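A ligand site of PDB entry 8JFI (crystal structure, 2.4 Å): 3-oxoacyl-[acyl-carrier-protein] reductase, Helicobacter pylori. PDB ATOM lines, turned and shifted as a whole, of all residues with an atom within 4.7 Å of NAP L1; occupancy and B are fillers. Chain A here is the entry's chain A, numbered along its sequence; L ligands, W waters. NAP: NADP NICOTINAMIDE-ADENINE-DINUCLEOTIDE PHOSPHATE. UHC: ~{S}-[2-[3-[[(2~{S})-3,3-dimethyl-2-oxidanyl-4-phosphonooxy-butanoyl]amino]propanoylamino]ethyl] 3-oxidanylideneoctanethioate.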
ATOM      1  N   THR A  12       9.835  -0.553 -10.146  1.00  0.00           N
ATOM      2  CA  THR A  12       9.736  -2.006  -9.997  1.00  0.00           C
ATOM      3  C   THR A  12       8.448  -2.371  -9.272  1.00  0.00           C
ATOM      4  O   THR A  12       7.997  -1.657  -8.368  1.00  0.00           O
ATOM      5  CB  THR A  12      10.941  -2.556  -9.246  1.00  0.00           C
ATOM      6  OG1 THR A  12      10.844  -2.225  -7.861  1.00  0.00           O
ATOM      7  CG2 THR A  12      12.211  -1.969  -9.817  1.00  0.00           C
ATOM      8  N   GLY A  13       7.839  -3.488  -9.666  1.00  0.00           N
ATOM      9  CA  GLY A  13       6.565  -3.899  -9.100  1.00  0.00           C
ATOM     10  C   GLY A  13       5.454  -2.877  -9.230  1.00  0.00           C
ATOM     11  O   GLY A  13       4.731  -2.654  -8.273  1.00  0.00           O
ATOM     12  N   SER A  15       2.692  -2.921 -11.231  1.00  0.00           N
ATOM     13  CA  SER A  15       1.445  -3.369 -11.865  1.00  0.00           C
ATOM     14  C   SER A  15       0.214  -2.997 -11.030  1.00  0.00           C
ATOM     15  O   SER A  15      -0.750  -2.430 -11.558  1.00  0.00           O
ATOM     16  CB  SER A  15       1.542  -4.859 -12.146  1.00  0.00           C
ATOM     17  OG  SER A  15       1.819  -5.562 -10.938  1.00  0.00           O
ATOM     18  N   LYS A  16       0.217  -3.293  -9.722  1.00  0.00           N
ATOM     19  CA  LYS A  16      -0.928  -3.012  -8.868  1.00  0.00           C
ATOM     20  C   LYS A  16      -0.478  -2.251  -7.626  1.00  0.00           C
ATOM     21  O   LYS A  16       0.712  -2.167  -7.312  1.00  0.00           O
ATOM     22  CB  LYS A  16      -1.651  -4.287  -8.413  1.00  0.00           C
ATOM     23  CG  LYS A  16      -0.770  -5.275  -7.677  1.00  0.00           C
ATOM     24  CD  LYS A  16      -1.441  -6.630  -7.591  1.00  0.00           C
ATOM     25  CE  LYS A  16      -1.886  -7.136  -8.968  1.00  0.00           C
ATOM     26  NZ  LYS A  16      -1.924  -8.641  -9.123  1.00  0.00           N
ATOM     27  N   GLY A  17      -1.468  -1.704  -6.907  1.00  0.00           N
ATOM     28  CA  GLY A  17      -1.216  -1.172  -5.584  1.00  0.00           C
ATOM     29  C   GLY A  17      -0.568   0.199  -5.649  1.00  0.00           C
ATOM     30  O   GLY A  17      -0.767   0.965  -6.594  1.00  0.00           O
ATOM     31  N   ILE A  18       0.212   0.503  -4.608  1.00  0.00           N
ATOM     32  CA  ILE A  18       0.937   1.776  -4.545  1.00  0.00           C
ATOM     33  C   ILE A  18       1.835   1.948  -5.773  1.00  0.00           C
ATOM     34  O   ILE A  18       2.063   3.074  -6.248  1.00  0.00           O
ATOM     35  CB  ILE A  18       1.794   1.851  -3.255  1.00  0.00           C
ATOM     36  CG1 ILE A  18       0.931   1.700  -1.998  1.00  0.00           C
ATOM     37  CG2 ILE A  18       2.601   3.128  -3.252  1.00  0.00           C
ATOM     38  CD1 ILE A  18       1.693   2.014  -0.746  1.00  0.00           C
ATOM     39  N   GLY A  19       2.394   0.847  -6.274  1.00  0.00           N
ATOM     40  CA  GLY A  19       3.222   0.938  -7.465  1.00  0.00           C
ATOM     41  C   GLY A  19       2.420   1.432  -8.650  1.00  0.00           C
ATOM     42  O   GLY A  19       2.905   2.257  -9.439  1.00  0.00           O
ATOM     43  N   ASN A  36       6.844  -2.033 -14.302  1.00  0.00           N
ATOM     44  CA  ASN A  36       7.405  -3.372 -14.187  1.00  0.00           C
ATOM     45  C   ASN A  36       6.384  -4.350 -13.630  1.00  0.00           C
ATOM     46  O   ASN A  36       5.617  -4.009 -12.708  1.00  0.00           O
ATOM     47  CB  ASN A  36       8.607  -3.364 -13.242  1.00  0.00           C
ATOM     48  CG  ASN A  36       9.177  -4.757 -13.019  1.00  0.00           C
ATOM     49  OD1 ASN A  36       8.804  -5.718 -13.682  1.00  0.00           O
ATOM     50  ND2 ASN A  36       9.985  -4.882 -11.960  1.00  0.00           N
ATOM     51  N   ARG A  38       6.241  -8.943 -12.799  1.00  0.00           N
ATOM     52  CA  ARG A  38       7.043 -10.161 -12.617  1.00  0.00           C
ATOM     53  C   ARG A  38       6.284 -11.301 -13.239  1.00  0.00           C
ATOM     54  O   ARG A  38       6.839 -12.122 -13.901  1.00  0.00           O
ATOM     55  CB  ARG A  38       6.987 -10.448 -11.121  1.00  0.00           C
ATOM     56  CG  ARG A  38       8.100 -11.222 -10.449  1.00  0.00           C
ATOM     57  CD  ARG A  38       7.636 -11.425  -9.012  1.00  0.00           C
ATOM     58  NE  ARG A  38       8.179 -12.256  -7.937  1.00  0.00           N
ATOM     59  CZ  ARG A  38       7.670 -12.309  -6.713  1.00  0.00           C
ATOM     60  NH1 ARG A  38       6.642 -11.582  -6.364  1.00  0.00           N
ATOM     61  NH2 ARG A  38       8.203 -13.092  -5.828  1.00  0.00           N
ATOM     62  N   SER A  39       4.982 -11.265 -13.067  1.00  0.00           N
ATOM     63  CA  SER A  39       4.267 -12.429 -13.575  1.00  0.00           C
ATOM     64  C   SER A  39       3.228 -12.105 -14.623  1.00  0.00           C
ATOM     65  O   SER A  39       3.612 -12.092 -15.758  1.00  0.00           O
ATOM     66  CB  SER A  39       3.813 -13.314 -12.468  1.00  0.00           C
ATOM     67  OG  SER A  39       2.513 -12.994 -12.038  1.00  0.00           O
ATOM     68  N   PHE A  63      10.557  -8.226 -15.516  1.00  0.00           N
ATOM     69  CA  PHE A  63      11.715  -8.802 -14.843  1.00  0.00           C
ATOM     70  C   PHE A  63      11.380  -9.053 -13.376  1.00  0.00           C
ATOM     71  O   PHE A  63      10.453  -8.452 -12.823  1.00  0.00           O
ATOM     72  CB  PHE A  63      12.972  -7.921 -15.008  1.00  0.00           C
ATOM     73  CG  PHE A  63      12.880  -6.561 -14.365  1.00  0.00           C
ATOM     74  CD1 PHE A  63      12.099  -5.585 -14.937  1.00  0.00           C
ATOM     75  CD2 PHE A  63      13.574  -6.263 -13.211  1.00  0.00           C
ATOM     76  CE1 PHE A  63      12.005  -4.341 -14.377  1.00  0.00           C
ATOM     77  CE2 PHE A  63      13.487  -5.004 -12.646  1.00  0.00           C
ATOM     78  CZ  PHE A  63      12.697  -4.046 -13.233  1.00  0.00           C
ATOM     79  N   ASP A  64      12.102 -10.007 -12.788  1.00  0.00           N
ATOM     80  CA  ASP A  64      12.118 -10.204 -11.342  1.00  0.00           C
ATOM     81  C   ASP A  64      13.178  -9.273 -10.774  1.00  0.00           C
ATOM     82  O   ASP A  64      14.377  -9.463 -11.041  1.00  0.00           O
ATOM     83  CB  ASP A  64      12.426 -11.649 -10.948  1.00  0.00           C
ATOM     84  CG  ASP A  64      12.460 -11.876  -9.412  1.00  0.00           C
ATOM     85  OD1 ASP A  64      12.937 -11.001  -8.629  1.00  0.00           O
ATOM     86  OD2 ASP A  64      12.003 -12.956  -8.969  1.00  0.00           O
ATOM     87  N   ALA A  65      12.732  -8.309  -9.972  1.00  0.00           N
ATOM     88  CA  ALA A  65      13.635  -7.309  -9.424  1.00  0.00           C
ATOM     89  C   ALA A  65      14.735  -7.943  -8.576  1.00  0.00           C
ATOM     90  O   ALA A  65      15.829  -7.369  -8.497  1.00  0.00           O
ATOM     91  CB  ALA A  65      12.837  -6.283  -8.634  1.00  0.00           C
ATOM     92  N   ALA A  66      14.492  -9.109  -7.982  1.00  0.00           N
ATOM     93  CA  ALA A  66      15.510  -9.802  -7.187  1.00  0.00           C
ATOM     94  C   ALA A  66      16.528 -10.529  -8.040  1.00  0.00           C
ATOM     95  O   ALA A  66      17.465 -11.114  -7.480  1.00  0.00           O
ATOM     96  CB  ALA A  66      14.867 -10.813  -6.240  1.00  0.00           C
ATOM     97  N   ASN A  91       9.942   0.090  -5.718  1.00  0.00           N
ATOM     98  CA  ASN A  91       8.692  -0.197  -5.023  1.00  0.00           C
ATOM     99  C   ASN A  91       8.502  -1.679  -4.700  1.00  0.00           C
ATOM    100  O   ASN A  91       7.818  -1.990  -3.719  1.00  0.00           O
ATOM    101  CB  ASN A  91       7.505   0.322  -5.864  1.00  0.00           C
ATOM    102  CG  ASN A  91       6.172  -0.182  -5.356  1.00  0.00           C
ATOM    103  OD1 ASN A  91       5.444  -0.880  -6.075  1.00  0.00           O
ATOM    104  ND2 ASN A  91       5.849   0.153  -4.118  1.00  0.00           N
ATOM    105  N   ALA A  92       9.138  -2.583  -5.461  1.00  0.00           N
ATOM    106  CA  ALA A  92       8.797  -4.007  -5.410  1.00  0.00           C
ATOM    107  C   ALA A  92       8.960  -4.558  -4.010  1.00  0.00           C
ATOM    108  O   ALA A  92      10.036  -4.453  -3.427  1.00  0.00           O
ATOM    109  CB  ALA A  92       9.684  -4.789  -6.359  1.00  0.00           C
ATOM    110  N   GLY A  93       7.893  -5.164  -3.494  1.00  0.00           N
ATOM    111  CA  GLY A  93       7.930  -5.679  -2.133  1.00  0.00           C
ATOM    112  C   GLY A  93       6.974  -6.825  -1.911  1.00  0.00           C
ATOM    113  O   GLY A  93       5.878  -6.886  -2.503  1.00  0.00           O
ATOM    114  N   VAL A  94       7.372  -7.747  -1.025  1.00  0.00           N
ATOM    115  CA  VAL A  94       6.543  -8.864  -0.604  1.00  0.00           C
ATOM    116  C   VAL A  94       6.447  -8.830   0.916  1.00  0.00           C
ATOM    117  O   VAL A  94       7.261  -8.211   1.598  1.00  0.00           O
ATOM    118  CB  VAL A  94       7.101 -10.226  -1.074  1.00  0.00           C
ATOM    119  CG1 VAL A  94       7.313 -10.226  -2.574  1.00  0.00           C
ATOM    120  CG2 VAL A  94       8.388 -10.517  -0.380  1.00  0.00           C
ATOM    121  N   ASN A 114      13.594 -10.451  -1.717  1.00  0.00           N
ATOM    122  CA  ASN A 114      12.699  -9.721  -2.611  1.00  0.00           C
ATOM    123  C   ASN A 114      12.607  -8.256  -2.239  1.00  0.00           C
ATOM    124  O   ASN A 114      12.497  -7.417  -3.128  1.00  0.00           O
ATOM    125  CB  ASN A 114      11.313 -10.326  -2.624  1.00  0.00           C
ATOM    126  CG  ASN A 114      11.184 -11.426  -3.656  1.00  0.00           C
ATOM    127  OD1 ASN A 114      11.003 -12.584  -3.287  1.00  0.00           O
ATOM    128  ND2 ASN A 114      11.275 -11.075  -4.954  1.00  0.00           N
ATOM    129  N   ILE A 141      10.651   2.723  -1.625  1.00  0.00           N
ATOM    130  CA  ILE A 141       9.466   2.566  -0.810  1.00  0.00           C
ATOM    131  C   ILE A 141       9.811   1.600   0.321  1.00  0.00           C
ATOM    132  O   ILE A 141       9.984   0.395   0.073  1.00  0.00           O
ATOM    133  CB  ILE A 141       8.284   2.033  -1.634  1.00  0.00           C
ATOM    134  CG1 ILE A 141       8.089   2.837  -2.918  1.00  0.00           C
ATOM    135  CG2 ILE A 141       7.006   2.099  -0.831  1.00  0.00           C
ATOM    136  CD1 ILE A 141       7.719   4.251  -2.679  1.00  0.00           C
ATOM    137  N   ALA A 142       9.937   2.125   1.555  1.00  0.00           N
ATOM    138  CA  ALA A 142      10.139   1.334   2.771  1.00  0.00           C
ATOM    139  C   ALA A 142       8.816   1.121   3.502  1.00  0.00           C
ATOM    140  O   ALA A 142       7.796   0.809   2.870  1.00  0.00           O
ATOM    141  CB  ALA A 142      11.147   1.999   3.708  1.00  0.00           C
ATOM    142  N   SER A 143       8.818   1.262   4.825  1.00  0.00           N
ATOM    143  CA  SER A 143       7.580   1.081   5.583  1.00  0.00           C
ATOM    144  C   SER A 143       7.754   1.575   7.007  1.00  0.00           C
ATOM    145  O   SER A 143       8.869   1.600   7.542  1.00  0.00           O
ATOM    146  CB  SER A 143       7.132  -0.378   5.644  1.00  0.00           C
ATOM    147  OG  SER A 143       6.021  -0.499   6.530  1.00  0.00           O
ATOM    148  N   TYR A 156      10.069  -8.836   7.421  1.00  0.00           N
ATOM    149  CA  TYR A 156       9.701  -7.606   6.739  1.00  0.00           C
ATOM    150  C   TYR A 156      10.409  -6.409   7.376  1.00  0.00           C
ATOM    151  O   TYR A 156      10.939  -5.547   6.673  1.00  0.00           O
ATOM    152  CB  TYR A 156       8.185  -7.455   6.794  1.00  0.00           C
ATOM    153  CG  TYR A 156       7.638  -6.317   5.993  1.00  0.00           C
ATOM    154  CD1 TYR A 156       7.508  -6.403   4.617  1.00  0.00           C
ATOM    155  CD2 TYR A 156       7.231  -5.156   6.627  1.00  0.00           C
ATOM    156  CE1 TYR A 156       6.979  -5.310   3.888  1.00  0.00           C
ATOM    157  CE2 TYR A 156       6.712  -4.078   5.912  1.00  0.00           C
ATOM    158  CZ  TYR A 156       6.600  -4.162   4.562  1.00  0.00           C
ATOM    159  OH  TYR A 156       6.082  -3.089   3.880  1.00  0.00           O
ATOM    160  N   LYS A 160      12.945  -3.774   5.500  1.00  0.00           N
ATOM    161  CA  LYS A 160      12.683  -2.340   5.353  1.00  0.00           C
ATOM    162  C   LYS A 160      13.762  -1.518   6.064  1.00  0.00           C
ATOM    163  O   LYS A 160      14.182  -0.465   5.572  1.00  0.00           O
ATOM    164  CB  LYS A 160      11.287  -2.011   5.885  1.00  0.00           C
ATOM    165  CG  LYS A 160      10.175  -2.768   5.183  1.00  0.00           C
ATOM    166  CD  LYS A 160      10.502  -2.864   3.720  1.00  0.00           C
ATOM    167  CE  LYS A 160       9.301  -2.668   2.855  1.00  0.00           C
ATOM    168  NZ  LYS A 160       9.808  -2.390   1.474  1.00  0.00           N
ATOM    169  N   PRO A 186       5.677   4.571   4.500  1.00  0.00           N
ATOM    170  CA  PRO A 186       4.232   4.798   4.668  1.00  0.00           C
ATOM    171  C   PRO A 186       3.673   4.147   5.910  1.00  0.00           C
ATOM    172  O   PRO A 186       4.247   3.226   6.497  1.00  0.00           O
ATOM    173  CB  PRO A 186       3.632   4.177   3.406  1.00  0.00           C
ATOM    174  CG  PRO A 186       4.806   4.002   2.453  1.00  0.00           C
ATOM    175  CD  PRO A 186       5.954   3.730   3.338  1.00  0.00           C
ATOM    176  N   GLY A 187       2.539   4.664   6.337  1.00  0.00           N
ATOM    177  CA  GLY A 187       1.810   4.026   7.408  1.00  0.00           C
ATOM    178  C   GLY A 187       0.992   2.904   6.836  1.00  0.00           C
ATOM    179  O   GLY A 187       1.520   2.066   6.099  1.00  0.00           O
ATOM    180  N   PHE A 188      -0.312   2.859   7.115  1.00  0.00           N
ATOM    181  CA  PHE A 188      -1.159   1.801   6.604  1.00  0.00           C
ATOM    182  C   PHE A 188      -2.080   2.289   5.497  1.00  0.00           C
ATOM    183  O   PHE A 188      -2.978   3.109   5.731  1.00  0.00           O
ATOM    184  CB  PHE A 188      -1.745   1.006   7.796  1.00  0.00           C
ATOM    185  CG  PHE A 188      -2.860   0.022   7.486  1.00  0.00           C
ATOM    186  CD1 PHE A 188      -2.928  -0.640   6.268  1.00  0.00           C
ATOM    187  CD2 PHE A 188      -3.377  -0.662   8.570  1.00  0.00           C
ATOM    188  CE1 PHE A 188      -3.916  -1.620   6.090  1.00  0.00           C
ATOM    189  CE2 PHE A 188      -4.275  -1.742   8.413  1.00  0.00           C
ATOM    190  CZ  PHE A 188      -4.530  -2.219   7.149  1.00  0.00           C
ATOM    191  N   ILE A 189      -1.759   1.822   4.265  1.00  0.00           N
ATOM    192  CA  ILE A 189      -2.316   2.254   2.997  1.00  0.00           C
ATOM    193  C   ILE A 189      -3.326   1.221   2.532  1.00  0.00           C
ATOM    194  O   ILE A 189      -3.128   0.011   2.724  1.00  0.00           O
ATOM    195  CB  ILE A 189      -1.220   2.446   1.936  1.00  0.00           C
ATOM    196  CG1 ILE A 189      -0.018   3.179   2.531  1.00  0.00           C
ATOM    197  CG2 ILE A 189      -1.728   3.232   0.771  1.00  0.00           C
ATOM    198  CD1 ILE A 189      -0.352   4.539   3.042  1.00  0.00           C
ATOM    199  N   THR A 191      -4.430  -0.798   0.205  1.00  0.00           N
ATOM    200  CA  THR A 191      -4.014  -1.439  -1.051  1.00  0.00           C
ATOM    201  C   THR A 191      -4.165  -2.962  -0.977  1.00  0.00           C
ATOM    202  O   THR A 191      -4.874  -3.509  -0.126  1.00  0.00           O
ATOM    203  CB  THR A 191      -2.572  -1.113  -1.467  1.00  0.00           C
ATOM    204  OG1 THR A 191      -1.637  -1.826  -0.639  1.00  0.00           O
ATOM    205  CG2 THR A 191      -2.327   0.389  -1.405  1.00  0.00           C
ATOM    206  N   ASP A 192      -3.463  -3.644  -1.897  1.00  0.00           N
ATOM    207  CA  ASP A 192      -3.599  -5.081  -2.105  1.00  0.00           C
ATOM    208  C   ASP A 192      -2.907  -5.874  -1.006  1.00  0.00           C
ATOM    209  O   ASP A 192      -3.382  -6.948  -0.613  1.00  0.00           O
ATOM    210  CB  ASP A 192      -3.040  -5.407  -3.508  1.00  0.00           C
ATOM    211  CG  ASP A 192      -3.141  -6.887  -3.911  1.00  0.00           C
ATOM    212  OD1 ASP A 192      -4.203  -7.299  -4.443  1.00  0.00           O
ATOM    213  OD2 ASP A 192      -2.130  -7.617  -3.769  1.00  0.00           O
ATOM    214  N   MET A 193      -1.816  -5.322  -0.455  1.00  0.00           N
ATOM    215  CA  MET A 193      -0.924  -6.090   0.418  1.00  0.00           C
ATOM    216  C   MET A 193      -1.560  -6.411   1.763  1.00  0.00           C
ATOM    217  O   MET A 193      -1.325  -7.492   2.313  1.00  0.00           O
ATOM    218  CB  MET A 193       0.385  -5.319   0.612  1.00  0.00           C
ATOM    219  CG  MET A 193       1.365  -6.016   1.533  1.00  0.00           C
ATOM    220  SD  MET A 193       2.723  -4.920   1.975  1.00  0.00           S
ATOM    221  CE  MET A 193       3.881  -5.392   0.664  1.00  0.00           C
ATOM    222  N   ASN A 194      -2.346  -5.493   2.306  1.00  0.00           N
ATOM    223  CA  ASN A 194      -2.984  -5.646   3.605  1.00  0.00           C
ATOM    224  C   ASN A 194      -4.509  -5.705   3.509  1.00  0.00           C
ATOM    225  O   ASN A 194      -5.173  -5.653   4.544  1.00  0.00           O
ATOM    226  CB  ASN A 194      -2.570  -4.486   4.510  1.00  0.00           C
ATOM    227  CG  ASN A 194      -2.841  -3.141   3.852  1.00  0.00           C
ATOM    228  OD1 ASN A 194      -3.959  -2.877   3.385  1.00  0.00           O
ATOM    229  ND2 ASN A 194      -1.833  -2.278   3.836  1.00  0.00           N
HETATM  230  PA  NAP L   1       1.070  -5.038  -3.583  1.00  0.00           P
HETATM  231  O1A NAP L   1      -0.308  -4.516  -3.838  1.00  0.00           O
HETATM  232  O2A NAP L   1       1.321  -6.474  -3.180  1.00  0.00           O
HETATM  233  O5B NAP L   1       2.074  -4.537  -4.734  1.00  0.00           O
HETATM  234  C5B NAP L   1       3.479  -5.049  -4.667  1.00  0.00           C
HETATM  235  C4B NAP L   1       3.972  -5.369  -6.058  1.00  0.00           C
HETATM  236  O4B NAP L   1       5.413  -5.629  -6.100  1.00  0.00           O
HETATM  237  C3B NAP L   1       3.266  -6.521  -6.814  1.00  0.00           C
HETATM  238  O3B NAP L   1       2.931  -6.170  -8.156  1.00  0.00           O
HETATM  239  C2B NAP L   1       4.360  -7.562  -6.802  1.00  0.00           C
HETATM  240  O2B NAP L   1       4.459  -8.933  -7.106  1.00  0.00           O
HETATM  241  C1B NAP L   1       5.567  -6.681  -7.021  1.00  0.00           C
HETATM  242  N9A NAP L   1       6.825  -7.382  -6.840  1.00  0.00           N
HETATM  243  C8A NAP L   1       7.231  -8.084  -5.753  1.00  0.00           C
HETATM  244  N7A NAP L   1       8.408  -8.625  -5.886  1.00  0.00           N
HETATM  245  C5A NAP L   1       8.778  -8.241  -7.143  1.00  0.00           C
HETATM  246  C6A NAP L   1       9.944  -8.497  -7.861  1.00  0.00           C
HETATM  247  N6A NAP L   1      10.908  -9.231  -7.329  1.00  0.00           N
HETATM  248  N1A NAP L   1      10.052  -7.985  -9.113  1.00  0.00           N
HETATM  249  C2A NAP L   1       9.032  -7.265  -9.588  1.00  0.00           C
HETATM  250  N3A NAP L   1       7.876  -6.963  -9.002  1.00  0.00           N
HETATM  251  C4A NAP L   1       7.822  -7.487  -7.768  1.00  0.00           C
HETATM  252  O3  NAP L   1       1.682  -4.121  -2.374  1.00  0.00           O
HETATM  253  PN  NAP L   1       1.567  -2.545  -2.008  1.00  0.00           P
HETATM  254  O1N NAP L   1       1.569  -2.494  -0.512  1.00  0.00           O
HETATM  255  O2N NAP L   1       0.384  -1.809  -2.594  1.00  0.00           O
HETATM  256  O5D NAP L   1       2.910  -1.909  -2.608  1.00  0.00           O
HETATM  257  C5D NAP L   1       4.193  -2.527  -2.456  1.00  0.00           C
HETATM  258  C4D NAP L   1       5.287  -1.723  -1.753  1.00  0.00           C
HETATM  259  O4D NAP L   1       4.821  -0.775  -0.816  1.00  0.00           O
HETATM  260  C3D NAP L   1       6.320  -2.577  -0.969  1.00  0.00           C
HETATM  261  O3D NAP L   1       7.672  -2.110  -0.952  1.00  0.00           O
HETATM  262  C2D NAP L   1       5.695  -2.592   0.437  1.00  0.00           C
HETATM  263  O2D NAP L   1       6.628  -3.408   1.199  1.00  0.00           O
HETATM  264  C1D NAP L   1       5.385  -1.047   0.459  1.00  0.00           C
HETATM  265  N1N NAP L   1       4.468  -0.523   1.528  1.00  0.00           N
HETATM  266  C2N NAP L   1       3.288  -1.189   1.819  1.00  0.00           C
HETATM  267  C3N NAP L   1       2.446  -0.674   2.834  1.00  0.00           C
HETATM  268  C7N NAP L   1       0.946  -0.918   2.763  1.00  0.00           C
HETATM  269  O7N NAP L   1       0.266  -0.822   3.768  1.00  0.00           O
HETATM  270  N7N NAP L   1       0.425  -1.241   1.593  1.00  0.00           N
HETATM  271  C4N NAP L   1       3.015   0.138   3.764  1.00  0.00           C
HETATM  272  C5N NAP L   1       4.370   0.320   3.679  1.00  0.00           C
HETATM  273  C6N NAP L   1       4.881   0.316   2.386  1.00  0.00           C
HETATM  274  P2B NAP L   1       3.438  -9.908  -7.827  1.00  0.00           P
HETATM  275  O1X NAP L   1       3.979 -10.534  -9.123  1.00  0.00           O
HETATM  276  O2X NAP L   1       3.453 -10.909  -6.686  1.00  0.00           O
HETATM  277  O3X NAP L   1       2.081  -9.151  -8.004  1.00  0.00           O
HETATM  278  C1  UHC L   2       2.401  -4.432   5.896  1.00  0.00           C
HETATM  279  O1  UHC L   2       3.118  -4.528   4.979  1.00  0.00           O
HETATM  280  S1  UHC L   2       0.888  -5.421   6.035  1.00  0.00           S
HETATM  281  C2  UHC L   2       2.594  -3.514   7.050  1.00  0.00           C
HETATM  282  C3  UHC L   2       2.735  -2.109   6.610  1.00  0.00           C
HETATM  283  O3  UHC L   2       3.666  -1.887   5.921  1.00  0.00           O
HETATM  284  C4  UHC L   2       1.730  -1.082   7.018  1.00  0.00           C
HETATM  285  C5  UHC L   2       1.108  -1.605   8.258  1.00  0.00           C
HETATM  286  C6  UHC L   2       1.056  -0.410   9.108  1.00  0.00           C
HETATM  287  O23 UHC L   2      -3.228 -14.264  16.837  1.00  0.00           O
HETATM  288  P24 UHC L   2      -2.332 -15.240  16.141  1.00  0.00           P
HETATM  289  O26 UHC L   2      -2.988 -16.454  15.287  1.00  0.00           O
HETATM  290  O27 UHC L   2      -1.271 -14.495  15.197  1.00  0.00           O
HETATM  291  C28 UHC L   2      -0.317 -13.685  15.851  1.00  0.00           C
HETATM  292  C29 UHC L   2      -0.391 -12.292  15.277  1.00  0.00           C
HETATM  293  C30 UHC L   2       0.429 -11.443  16.274  1.00  0.00           C
HETATM  294  C31 UHC L   2      -1.862 -11.902  15.426  1.00  0.00           C
HETATM  295  C32 UHC L   2       0.033 -12.276  13.763  1.00  0.00           C
HETATM  296  O33 UHC L   2       0.865 -13.368  13.365  1.00  0.00           O
HETATM  297  C34 UHC L   2       0.694 -10.950  13.317  1.00  0.00           C
HETATM  298  O35 UHC L   2       1.861 -10.748  13.665  1.00  0.00           O
HETATM  299  N36 UHC L   2      -0.002 -10.078  12.524  1.00  0.00           N
HETATM  300  C37 UHC L   2       0.615  -8.824  12.096  1.00  0.00           C
HETATM  301  C38 UHC L   2      -0.035  -8.280  10.815  1.00  0.00           C
HETATM  302  C39 UHC L   2       0.066  -6.763  10.828  1.00  0.00           C
HETATM  303  O40 UHC L   2      -0.028  -6.146  11.900  1.00  0.00           O
HETATM  304  N41 UHC L   2       0.241  -6.176   9.637  1.00  0.00           N
HETATM  305  C42 UHC L   2       0.324  -6.926   8.361  1.00  0.00           C
HETATM  306  C43 UHC L   2       1.471  -6.375   7.485  1.00  0.00           C
HETATM  307  O   HOH W   1       2.360  -1.688  -5.181  1.00  0.00           O
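O of Phe 63 lies close to OD1 of Asn 36 (3.3 Å).
The side-chain amide oxygen of Asn 91 sits close to the backbone carbonyl oxygen of Gly 13.
The backbone NH (N) of Ala 92 lies within hydrogen-bond range of the side-chain hydroxyl (OG1) of Thr 12, at 3.0 Å.
The backbone NH (N) of Ser 15 lies within hydrogen-bond range of the backbone carbonyl oxygen (O) of Asn 36.
The backbone NH (N) of Gly 13 sits close to the side-chain amide nitrogen (ND2) of Asn 36 (3.4 Å).
ND2 of Asn 194 is in hydrogen-bond range of O of Ile 189, at 2.9 Å.
The side-chain amino group (NZ) of Lys 160 sits at hydrogen-bond distance from the backbone carbonyl oxygen (O) of Ile 141, at 3.1 Å.
The side-chain hydroxyl (OG1) of Thr 12 sits at hydrogen-bond distance from the backbone NH (N) of Asn 91 (3.3 Å).
The side-chain sulfur of Met 193 sits close to an oxygen (O1N) of NAP L1 (3.7 Å).
Gly 13 touches NAP L1 (CA to N3A, 3.3 Å).
O of Lys 16 touches O5B of NAP L1, at 3.8 Å.
Gly 17 touches NAP L1.
ND2 of Asn 36 touches C2A of NAP L1 (3.5 Å).
O of Phe 63 touches C2A of NAP L1, 3.7 Å away.
Ala 66 touches NAP L1 (N to N6A, 3.6 Å).
CB of Ala 92 touches C4A of NAP L1 (3.6 Å).
Gly 93 touches NAP L1.
Val 94 touches NAP L1.
Ile 141 touches NAP L1.
O of Ala 142 touches C6N of NAP L1, 3.0 Å away.
Ser 143 touches NAP L1 (OG to C5N, 3.4 Å).
CG of Pro 186 touches C6N of NAP L1, at 3.7 Å.
Gly 187 touches NAP L1.
Asp 192 touches NAP L1.
Hydrophobic or aromatic side chains within 4 Å of NAP L1: Ile 18, Ala 65, Ala 92, Val 94, Ile 141, Tyr 156, Pro 186 and Met 193.
The side-chain hydroxyl of Tyr 156 lies within hydrogen-bond range of an oxygen (O2D) of NAP L1 (2.8 Å).
The backbone NH (N) of Ile 189 is in hydrogen-bond range of an oxygen (O7N) of NAP L1.
O of Asn 91 sits at hydrogen-bond distance from O3D of NAP L1 (2.8 Å).
The backbone NH of Ala 65 lies within hydrogen-bond range of a nitrogen (N1A) of NAP L1 (2.8 Å).
An oxygen (O7N) of NAP L1 lies within hydrogen-bond range of the side-chain amide nitrogen (ND2) of Asn 194 (2.6 Å).
The side-chain hydroxyl of Ser 143 is in hydrogen-bond range of an oxygen (O3) of UHC L2 (2.8 Å).
The backbone NH (N) of Ile 18 is in hydrogen-bond range of an oxygen (O2N) of NAP L1 (3.1 Å).
OH of Tyr 156 is in hydrogen-bond range of O3 of UHC L2 (3.4 Å).
ND2 of Asn 114 lies close to N6A of NAP L1.
A nitrogen (N6A) of NAP L1 lies within hydrogen-bond range of the side-chain carboxylate (OD1) of Asp 64.
The side-chain hydroxyl (OG) of Ser 15 lies within hydrogen-bond range of an oxygen (O3B) of NAP L1, at 3.1 Å.
The side-chain amino group (NZ) of Lys 160 lies within hydrogen-bond range of an oxygen (O3D) of NAP L1, 3.2 Å away.
The side-chain hydroxyl of Thr 191 is in hydrogen-bond range of an oxygen (O2N) of NAP L1 (2.8 Å).
O2X of NAP L1 lies within salt-bridge range of NH1 of Arg 38 (3.3 Å).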
